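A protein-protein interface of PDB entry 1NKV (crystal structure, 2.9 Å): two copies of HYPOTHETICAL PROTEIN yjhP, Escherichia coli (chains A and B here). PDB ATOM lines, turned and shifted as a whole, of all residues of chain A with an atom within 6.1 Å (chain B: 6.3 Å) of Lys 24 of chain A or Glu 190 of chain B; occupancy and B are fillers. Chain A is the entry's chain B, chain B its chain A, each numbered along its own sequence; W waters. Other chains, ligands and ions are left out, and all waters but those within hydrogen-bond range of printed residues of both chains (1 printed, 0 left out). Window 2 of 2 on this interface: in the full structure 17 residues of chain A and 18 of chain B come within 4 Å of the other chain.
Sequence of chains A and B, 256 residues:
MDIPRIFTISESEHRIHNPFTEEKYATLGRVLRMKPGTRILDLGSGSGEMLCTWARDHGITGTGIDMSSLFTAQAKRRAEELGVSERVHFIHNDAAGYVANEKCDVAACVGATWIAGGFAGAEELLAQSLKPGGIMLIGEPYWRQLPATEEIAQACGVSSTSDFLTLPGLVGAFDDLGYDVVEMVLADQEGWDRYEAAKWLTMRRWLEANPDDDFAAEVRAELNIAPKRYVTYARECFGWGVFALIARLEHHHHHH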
ATOM      1  N   PHE A  20     -10.892   5.114   1.140  1.00  0.00           N
ATOM      2  CA  PHE A  20     -12.012   4.263   0.738  1.00  0.00           C
ATOM      3  C   PHE A  20     -13.103   4.952  -0.061  1.00  0.00           C
ATOM      4  O   PHE A  20     -13.339   6.143   0.088  1.00  0.00           O
ATOM      5  CB  PHE A  20     -12.620   3.586   1.967  1.00  0.00           C
ATOM      6  CG  PHE A  20     -12.171   2.150   2.159  1.00  0.00           C
ATOM      7  CD1 PHE A  20     -10.957   1.701   1.640  1.00  0.00           C
ATOM      8  CD2 PHE A  20     -12.949   1.262   2.897  1.00  0.00           C
ATOM      9  CE1 PHE A  20     -10.535   0.393   1.859  1.00  0.00           C
ATOM     10  CE2 PHE A  20     -12.534  -0.043   3.120  1.00  0.00           C
ATOM     11  CZ  PHE A  20     -11.329  -0.475   2.603  1.00  0.00           C
ATOM     12  N   THR A  21     -13.752   4.196  -0.941  1.00  0.00           N
ATOM     13  CA  THR A  21     -14.846   4.749  -1.732  1.00  0.00           C
ATOM     14  C   THR A  21     -16.128   4.142  -1.218  1.00  0.00           C
ATOM     15  O   THR A  21     -16.118   3.266  -0.357  1.00  0.00           O
ATOM     16  CB  THR A  21     -14.775   4.406  -3.245  1.00  0.00           C
ATOM     17  OG1 THR A  21     -15.182   3.055  -3.449  1.00  0.00           O
ATOM     18  CG2 THR A  21     -13.378   4.605  -3.796  1.00  0.00           C
ATOM     19  N   GLU A  22     -17.241   4.600  -1.757  1.00  0.00           N
ATOM     20  CA  GLU A  22     -18.511   4.070  -1.343  1.00  0.00           C
ATOM     21  C   GLU A  22     -18.493   2.568  -1.648  1.00  0.00           C
ATOM     22  O   GLU A  22     -18.838   1.758  -0.790  1.00  0.00           O
ATOM     23  CB  GLU A  22     -19.624   4.776  -2.107  1.00  0.00           C
ATOM     24  CG  GLU A  22     -20.946   4.805  -1.374  1.00  0.00           C
ATOM     25  CD  GLU A  22     -20.864   5.555  -0.052  1.00  0.00           C
ATOM     26  OE1 GLU A  22     -20.417   6.726  -0.062  1.00  0.00           O
ATOM     27  OE2 GLU A  22     -21.249   4.980   0.996  1.00  0.00           O
ATOM     28  N   GLU A  23     -18.048   2.214  -2.858  1.00  0.00           N
ATOM     29  CA  GLU A  23     -17.990   0.827  -3.333  1.00  0.00           C
ATOM     30  C   GLU A  23     -17.067  -0.035  -2.491  1.00  0.00           C
ATOM     31  O   GLU A  23     -17.286  -1.241  -2.354  1.00  0.00           O
ATOM     32  CB  GLU A  23     -17.528   0.798  -4.800  1.00  0.00           C
ATOM     33  CG  GLU A  23     -17.962  -0.416  -5.618  1.00  0.00           C
ATOM     34  CD  GLU A  23     -17.160  -1.681  -5.311  1.00  0.00           C
ATOM     35  OE1 GLU A  23     -15.910  -1.641  -5.459  1.00  0.00           O
ATOM     36  OE2 GLU A  23     -17.775  -2.714  -4.929  1.00  0.00           O
ATOM     37  N   LYS A  24     -16.044   0.589  -1.918  1.00  0.00           N
ATOM     38  CA  LYS A  24     -15.068  -0.118  -1.095  1.00  0.00           C
ATOM     39  C   LYS A  24     -15.657  -0.556   0.235  1.00  0.00           C
ATOM     40  O   LYS A  24     -15.397  -1.667   0.702  1.00  0.00           O
ATOM     41  CB  LYS A  24     -13.860   0.770  -0.834  1.00  0.00           C
ATOM     42  CG  LYS A  24     -12.553   0.095  -1.132  1.00  0.00           C
ATOM     43  CD  LYS A  24     -12.368  -0.077  -2.624  1.00  0.00           C
ATOM     44  CE  LYS A  24     -11.058  -0.770  -2.921  1.00  0.00           C
ATOM     45  NZ  LYS A  24     -10.860  -0.979  -4.372  1.00  0.00           N
ATOM     46  N   TYR A  25     -16.439   0.322   0.854  1.00  0.00           N
ATOM     47  CA  TYR A  25     -17.063  -0.021   2.120  1.00  0.00           C
ATOM     48  C   TYR A  25     -18.121  -1.107   1.926  1.00  0.00           C
ATOM     49  O   TYR A  25     -18.348  -1.915   2.808  1.00  0.00           O
ATOM     50  CB  TYR A  25     -17.721   1.204   2.773  1.00  0.00           C
ATOM     51  CG  TYR A  25     -16.849   1.959   3.760  1.00  0.00           C
ATOM     52  CD1 TYR A  25     -16.176   1.297   4.791  1.00  0.00           C
ATOM     53  CD2 TYR A  25     -16.720   3.342   3.677  1.00  0.00           C
ATOM     54  CE1 TYR A  25     -15.397   1.998   5.711  1.00  0.00           C
ATOM     55  CE2 TYR A  25     -15.950   4.048   4.584  1.00  0.00           C
ATOM     56  CZ  TYR A  25     -15.292   3.378   5.594  1.00  0.00           C
ATOM     57  OH  TYR A  25     -14.525   4.105   6.473  1.00  0.00           O
ATOM     58  N   ALA A  26     -18.776  -1.137   0.777  1.00  0.00           N
ATOM     59  CA  ALA A  26     -19.789  -2.157   0.579  1.00  0.00           C
ATOM     60  C   ALA A  26     -19.150  -3.534   0.340  1.00  0.00           C
ATOM     61  O   ALA A  26     -19.729  -4.551   0.729  1.00  0.00           O
ATOM     62  CB  ALA A  26     -20.720  -1.770  -0.593  1.00  0.00           C
ATOM     63  N   THR A  27     -17.978  -3.554  -0.312  1.00  0.00           N
ATOM     64  CA  THR A  27     -17.237  -4.793  -0.612  1.00  0.00           C
ATOM     65  C   THR A  27     -16.671  -5.452   0.647  1.00  0.00           C
ATOM     66  O   THR A  27     -16.647  -6.675   0.764  1.00  0.00           O
ATOM     67  CB  THR A  27     -16.053  -4.541  -1.589  1.00  0.00           C
ATOM     68  OG1 THR A  27     -16.560  -4.347  -2.910  1.00  0.00           O
ATOM     69  CG2 THR A  27     -15.092  -5.710  -1.590  1.00  0.00           C
ATOM     70  N   LEU A  28     -16.201  -4.623   1.576  1.00  0.00           N
ATOM     71  CA  LEU A  28     -15.647  -5.111   2.821  1.00  0.00           C
ATOM     72  C   LEU A  28     -16.806  -5.822   3.534  1.00  0.00           C
ATOM     73  O   LEU A  28     -16.683  -6.961   3.977  1.00  0.00           O
ATOM     74  CB  LEU A  28     -15.127  -3.938   3.648  1.00  0.00           C
ATOM     75  CG  LEU A  28     -14.162  -4.152   4.826  1.00  0.00           C
ATOM     76  CD1 LEU A  28     -14.361  -3.009   5.836  1.00  0.00           C
ATOM     77  CD2 LEU A  28     -14.421  -5.476   5.494  1.00  0.00           C
ATOM     78  N   GLY A  29     -17.946  -5.160   3.616  1.00  0.00           N
ATOM     79  CA  GLY A  29     -19.084  -5.776   4.256  1.00  0.00           C
ATOM     80  C   GLY A  29     -19.449  -7.152   3.720  1.00  0.00           C
ATOM     81  O   GLY A  29     -19.513  -8.106   4.493  1.00  0.00           O
ATOM     82  N   VAL A 185      -9.262  -5.447   2.551  1.00  0.00           N
ATOM     83  CA  VAL A 185      -9.718  -4.568   1.481  1.00  0.00           C
ATOM     84  C   VAL A 185      -8.922  -3.285   1.485  1.00  0.00           C
ATOM     85  O   VAL A 185      -9.123  -2.434   2.345  1.00  0.00           O
ATOM     86  CB  VAL A 185     -11.176  -4.208   1.632  1.00  0.00           C
ATOM     87  CG1 VAL A 185     -11.510  -3.118   0.640  1.00  0.00           C
ATOM     88  CG2 VAL A 185     -12.042  -5.439   1.394  1.00  0.00           C
ATOM     89  N   LEU A 186      -8.021  -3.153   0.518  1.00  0.00           N
ATOM     90  CA  LEU A 186      -7.164  -1.973   0.403  1.00  0.00           C
ATOM     91  C   LEU A 186      -7.738  -0.938  -0.552  1.00  0.00           C
ATOM     92  O   LEU A 186      -8.628  -1.228  -1.339  1.00  0.00           O
ATOM     93  CB  LEU A 186      -5.792  -2.375  -0.116  1.00  0.00           C
ATOM     94  CG  LEU A 186      -5.252  -3.601   0.599  1.00  0.00           C
ATOM     95  CD1 LEU A 186      -4.072  -4.175  -0.153  1.00  0.00           C
ATOM     96  CD2 LEU A 186      -4.913  -3.210   2.006  1.00  0.00           C
ATOM     97  N   ALA A 187      -7.185   0.266  -0.488  1.00  0.00           N
ATOM     98  CA  ALA A 187      -7.610   1.355  -1.333  1.00  0.00           C
ATOM     99  C   ALA A 187      -6.742   1.420  -2.601  1.00  0.00           C
ATOM    100  O   ALA A 187      -5.608   0.929  -2.622  1.00  0.00           O
ATOM    101  CB  ALA A 187      -7.520   2.653  -0.565  1.00  0.00           C
ATOM    102  N   ASP A 188      -7.275   2.032  -3.658  1.00  0.00           N
ATOM    103  CA  ASP A 188      -6.557   2.172  -4.922  1.00  0.00           C
ATOM    104  C   ASP A 188      -6.412   3.645  -5.297  1.00  0.00           C
ATOM    105  O   ASP A 188      -7.089   4.493  -4.722  1.00  0.00           O
ATOM    106  CB  ASP A 188      -7.313   1.425  -6.013  1.00  0.00           C
ATOM    107  CG  ASP A 188      -8.729   1.927  -6.183  1.00  0.00           C
ATOM    108  OD1 ASP A 188      -9.335   2.365  -5.179  1.00  0.00           O
ATOM    109  OD2 ASP A 188      -9.252   1.868  -7.323  1.00  0.00           O
ATOM    110  N   PRO B  19      -8.283 -14.099 -10.488  1.00  0.00           N
ATOM    111  CA  PRO B  19      -8.259 -12.672 -10.153  1.00  0.00           C
ATOM    112  C   PRO B  19      -9.393 -11.842 -10.764  1.00  0.00           C
ATOM    113  O   PRO B  19      -9.592 -10.705 -10.374  1.00  0.00           O
ATOM    114  CB  PRO B  19      -6.890 -12.219 -10.656  1.00  0.00           C
ATOM    115  CG  PRO B  19      -6.053 -13.436 -10.460  1.00  0.00           C
ATOM    116  CD  PRO B  19      -6.953 -14.564 -10.923  1.00  0.00           C
ATOM    117  N   THR B  21     -13.156 -10.236 -11.681  1.00  0.00           N
ATOM    118  CA  THR B  21     -14.248  -9.863 -10.791  1.00  0.00           C
ATOM    119  C   THR B  21     -15.551  -9.909 -11.560  1.00  0.00           C
ATOM    120  O   THR B  21     -15.570 -10.091 -12.778  1.00  0.00           O
ATOM    121  CB  THR B  21     -14.124  -8.427 -10.226  1.00  0.00           C
ATOM    122  OG1 THR B  21     -14.106  -7.482 -11.306  1.00  0.00           O
ATOM    123  CG2 THR B  21     -12.900  -8.280  -9.378  1.00  0.00           C
ATOM    124  N   ASP B 188      -6.767  -6.740 -12.265  1.00  0.00           N
ATOM    125  CA  ASP B 188      -6.045  -5.737 -11.511  1.00  0.00           C
ATOM    126  C   ASP B 188      -5.846  -6.198 -10.068  1.00  0.00           C
ATOM    127  O   ASP B 188      -6.629  -6.990  -9.545  1.00  0.00           O
ATOM    128  CB  ASP B 188      -6.806  -4.418 -11.562  1.00  0.00           C
ATOM    129  CG  ASP B 188      -8.192  -4.530 -10.991  1.00  0.00           C
ATOM    130  OD1 ASP B 188      -9.052  -3.691 -11.339  1.00  0.00           O
ATOM    131  OD2 ASP B 188      -8.431  -5.451 -10.186  1.00  0.00           O
ATOM    132  N   GLN B 189      -4.782  -5.706  -9.442  1.00  0.00           N
ATOM    133  CA  GLN B 189      -4.455  -6.043  -8.069  1.00  0.00           C
ATOM    134  C   GLN B 189      -5.680  -6.231  -7.171  1.00  0.00           C
ATOM    135  O   GLN B 189      -5.737  -7.182  -6.378  1.00  0.00           O
ATOM    136  CB  GLN B 189      -3.542  -4.974  -7.483  1.00  0.00           C
ATOM    137  CG  GLN B 189      -2.081  -5.198  -7.773  1.00  0.00           C
ATOM    138  CD  GLN B 189      -1.221  -4.008  -7.398  1.00  0.00           C
ATOM    139  OE1 GLN B 189      -0.006  -4.117  -7.332  1.00  0.00           O
ATOM    140  NE2 GLN B 189      -1.850  -2.864  -7.164  1.00  0.00           N
ATOM    141  N   GLU B 190      -6.653  -5.330  -7.289  1.00  0.00           N
ATOM    142  CA  GLU B 190      -7.881  -5.412  -6.497  1.00  0.00           C
ATOM    143  C   GLU B 190      -8.528  -6.767  -6.721  1.00  0.00           C
ATOM    144  O   GLU B 190      -8.906  -7.439  -5.765  1.00  0.00           O
ATOM    145  CB  GLU B 190      -8.860  -4.312  -6.919  1.00  0.00           C
ATOM    146  CG  GLU B 190     -10.250  -4.425  -6.305  1.00  0.00           C
ATOM    147  CD  GLU B 190     -10.231  -4.306  -4.792  1.00  0.00           C
ATOM    148  OE1 GLU B 190      -9.230  -3.747  -4.262  1.00  0.00           O
ATOM    149  OE2 GLU B 190     -11.214  -4.756  -4.130  1.00  0.00           O
ATOM    150  N   GLY B 191      -8.648  -7.150  -7.992  1.00  0.00           N
ATOM    151  CA  GLY B 191      -9.245  -8.421  -8.355  1.00  0.00           C
ATOM    152  C   GLY B 191      -8.474  -9.579  -7.753  1.00  0.00           C
ATOM    153  O   GLY B 191      -9.019 -10.647  -7.472  1.00  0.00           O
ATOM    154  N   TRP B 192      -7.181  -9.360  -7.572  1.00  0.00           N
ATOM    155  CA  TRP B 192      -6.350 -10.363  -6.968  1.00  0.00           C
ATOM    156  C   TRP B 192      -6.702 -10.414  -5.494  1.00  0.00           C
ATOM    157  O   TRP B 192      -6.939 -11.486  -4.965  1.00  0.00           O
ATOM    158  CB  TRP B 192      -4.868 -10.034  -7.136  1.00  0.00           C
ATOM    159  CG  TRP B 192      -4.238 -10.653  -8.335  1.00  0.00           C
ATOM    160  CD1 TRP B 192      -4.075 -10.085  -9.560  1.00  0.00           C
ATOM    161  CD2 TRP B 192      -3.706 -11.976  -8.433  1.00  0.00           C
ATOM    162  NE1 TRP B 192      -3.470 -10.971 -10.423  1.00  0.00           N
ATOM    163  CE2 TRP B 192      -3.233 -12.142  -9.754  1.00  0.00           C
ATOM    164  CE3 TRP B 192      -3.583 -13.041  -7.532  1.00  0.00           C
ATOM    165  CZ2 TRP B 192      -2.645 -13.335 -10.200  1.00  0.00           C
ATOM    166  CZ3 TRP B 192      -2.998 -14.230  -7.978  1.00  0.00           C
ATOM    167  CH2 TRP B 192      -2.538 -14.361  -9.302  1.00  0.00           C
ATOM    168  N   ASP B 193      -6.785  -9.272  -4.819  1.00  0.00           N
ATOM    169  CA  ASP B 193      -7.090  -9.334  -3.393  1.00  0.00           C
ATOM    170  C   ASP B 193      -8.349 -10.113  -3.062  1.00  0.00           C
ATOM    171  O   ASP B 193      -8.348 -10.963  -2.176  1.00  0.00           O
ATOM    172  CB  ASP B 193      -7.232  -7.949  -2.784  1.00  0.00           C
ATOM    173  CG  ASP B 193      -5.957  -7.190  -2.793  1.00  0.00           C
ATOM    174  OD1 ASP B 193      -4.895  -7.805  -2.559  1.00  0.00           O
ATOM    175  OD2 ASP B 193      -6.010  -5.965  -3.025  1.00  0.00           O
ATOM    176  N   ARG B 194      -9.431  -9.802  -3.761  1.00  0.00           N
ATOM    177  CA  ARG B 194     -10.693 -10.469  -3.517  1.00  0.00           C
ATOM    178  C   ARG B 194     -10.533 -11.984  -3.678  1.00  0.00           C
ATOM    179  O   ARG B 194     -11.189 -12.762  -2.989  1.00  0.00           O
ATOM    180  CB  ARG B 194     -11.759  -9.925  -4.476  1.00  0.00           C
ATOM    181  CG  ARG B 194     -12.113  -8.441  -4.284  1.00  0.00           C
ATOM    182  CD  ARG B 194     -12.879  -8.195  -2.980  1.00  0.00           C
ATOM    183  NE  ARG B 194     -12.090  -8.596  -1.815  1.00  0.00           N
ATOM    184  CZ  ARG B 194     -10.955  -8.008  -1.442  1.00  0.00           C
ATOM    185  NH1 ARG B 194     -10.473  -6.978  -2.128  1.00  0.00           N
ATOM    186  NH2 ARG B 194     -10.277  -8.486  -0.415  1.00  0.00           N
ATOM    187  N   TYR B 195      -9.633 -12.389  -4.570  1.00  0.00           N
ATOM    188  CA  TYR B 195      -9.383 -13.792  -4.835  1.00  0.00           C
ATOM    189  C   TYR B 195      -8.572 -14.485  -3.731  1.00  0.00           C
ATOM    190  O   TYR B 195      -8.983 -15.530  -3.217  1.00  0.00           O
ATOM    191  CB  TYR B 195      -8.695 -13.928  -6.201  1.00  0.00           C
ATOM    192  CG  TYR B 195      -8.334 -15.339  -6.588  1.00  0.00           C
ATOM    193  CD1 TYR B 195      -9.294 -16.347  -6.588  1.00  0.00           C
ATOM    194  CD2 TYR B 195      -7.020 -15.679  -6.897  1.00  0.00           C
ATOM    195  CE1 TYR B 195      -8.952 -17.656  -6.868  1.00  0.00           C
ATOM    196  CE2 TYR B 195      -6.666 -16.984  -7.180  1.00  0.00           C
ATOM    197  CZ  TYR B 195      -7.631 -17.967  -7.159  1.00  0.00           C
ATOM    198  OH  TYR B 195      -7.269 -19.275  -7.397  1.00  0.00           O
ATOM    199  N   TYR B 230       1.540 -13.773  -0.220  1.00  0.00           N
ATOM    200  CA  TYR B 230       0.916 -12.946  -1.230  1.00  0.00           C
ATOM    201  C   TYR B 230       1.372 -11.487  -1.188  1.00  0.00           C
ATOM    202  O   TYR B 230       2.005 -10.999  -2.124  1.00  0.00           O
ATOM    203  CB  TYR B 230      -0.593 -13.042  -1.077  1.00  0.00           C
ATOM    204  CG  TYR B 230      -1.368 -12.048  -1.901  1.00  0.00           C
ATOM    205  CD1 TYR B 230      -1.363 -12.098  -3.301  1.00  0.00           C
ATOM    206  CD2 TYR B 230      -2.157 -11.079  -1.273  1.00  0.00           C
ATOM    207  CE1 TYR B 230      -2.141 -11.203  -4.048  1.00  0.00           C
ATOM    208  CE2 TYR B 230      -2.929 -10.193  -2.003  1.00  0.00           C
ATOM    209  CZ  TYR B 230      -2.918 -10.257  -3.384  1.00  0.00           C
ATOM    210  OH  TYR B 230      -3.671  -9.359  -4.076  1.00  0.00           O
ATOM    211  N   ARG B 235       1.460 -10.316  -5.185  1.00  0.00           N
ATOM    212  CA  ARG B 235       0.669  -9.109  -5.436  1.00  0.00           C
ATOM    213  C   ARG B 235       1.324  -8.044  -6.300  1.00  0.00           C
ATOM    214  O   ARG B 235       0.666  -7.098  -6.725  1.00  0.00           O
ATOM    215  CB  ARG B 235       0.260  -8.481  -4.104  1.00  0.00           C
ATOM    216  CG  ARG B 235      -0.695  -7.338  -4.260  1.00  0.00           C
ATOM    217  CD  ARG B 235      -1.313  -6.954  -2.945  1.00  0.00           C
ATOM    218  NE  ARG B 235      -2.450  -6.059  -3.137  1.00  0.00           N
ATOM    219  CZ  ARG B 235      -2.371  -4.813  -3.601  1.00  0.00           C
ATOM    220  NH1 ARG B 235      -1.199  -4.285  -3.933  1.00  0.00           N
ATOM    221  NH2 ARG B 235      -3.472  -4.090  -3.737  1.00  0.00           N
HETATM  222  O   HOH W   1      -8.152  -5.146  -1.738  1.00  0.00           O
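The backbone carbonyl oxygen (O) of Arg 235 of chain B sits close to the side-chain amide oxygen (OE1) of Gln 189 of chain B, at 3.1 Å. The guanidinium group (NH1) of Arg 194 of chain B is in salt-bridge range of the side-chain carboxylate (OE2) of Glu 190 of chain B (3.1 Å). The side-chain carboxylate (OD1) of Asp 193 of chain B lies within hydrogen-bond range of the side-chain hydroxyl (OH) of Tyr 230 of chain B, at 2.5 Å. The guanidinium group (NE) of Arg 235 of chain B lies within salt-bridge range of the side-chain carboxylate (OD1) of Asp 193 of chain B. OG1 of Thr 21 of chain A lies within hydrogen-bond range of N of Lys 24 of chain A, at 3.0 Å. The side-chain amino group (NZ) of Lys 24 of chain A lies within salt-bridge range of the side-chain carboxylate (OD1) of Asp 188 of chain A (3.8 Å).
Water W1 lies within hydrogen-bond range of OD2 of Asp 193 of chain B (2.6 Å), NH1 of Arg 194 of chain B (3.0 Å), N of Leu 186 of chain A (3.0 Å) and OE1 of Glu 190 of chain B (3.1 Å).
Of the 12 printed residues of chain B, 4 touch a printed residue of chain A. Along chain B the printed residues that touch a printed residue of chain A span positions 190 to 235. Hydrophobic or aromatic side chains of chain A that line the printed part of chain B: Val 185 and Leu 186. Among the printed residues, 6 pairs touch across the chains.
Arg 194 of chain B touches Thr 27 of chain A. Val 185 of chain A touches Arg 194 of chain B. Glu 190 of chain B touches Leu 186 of chain A. Asp 193 of chain B touches Leu 186 of chain A. Leu 186 of chain A touches Arg 235 of chain B (CD1 to NH2, 3.6 Å).
The side-chain carboxylate (OE1) of Glu 190 of chain B is in salt-bridge range of the side-chain amino group (NZ) of Lys 24 of chain A (3.2 Å).
Positions printed for both chains: 21 and 188.
Of chain B, only Glu 190 comes within 4 Å of Lys 24 of chain A. Printed residues of chain B within 4 Å of Thr 27 of chain A: Arg 194. Of the printed residues of chain B, Val 185 of chain A touches Arg 194 (3.96 Å). Of the printed residues of chain B, Leu 186 of chain A touches Glu 190 (3.9 Å), Asp 193 (3.9 Å) and Arg 235 (3.6 Å). Glu 190 of chain B touches just these residues of chain A: Lys 24 (3.2 Å) and Leu 186 (3.9 Å). Of the printed residues of chain A, Asp 193 of chain B touches Leu 186.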
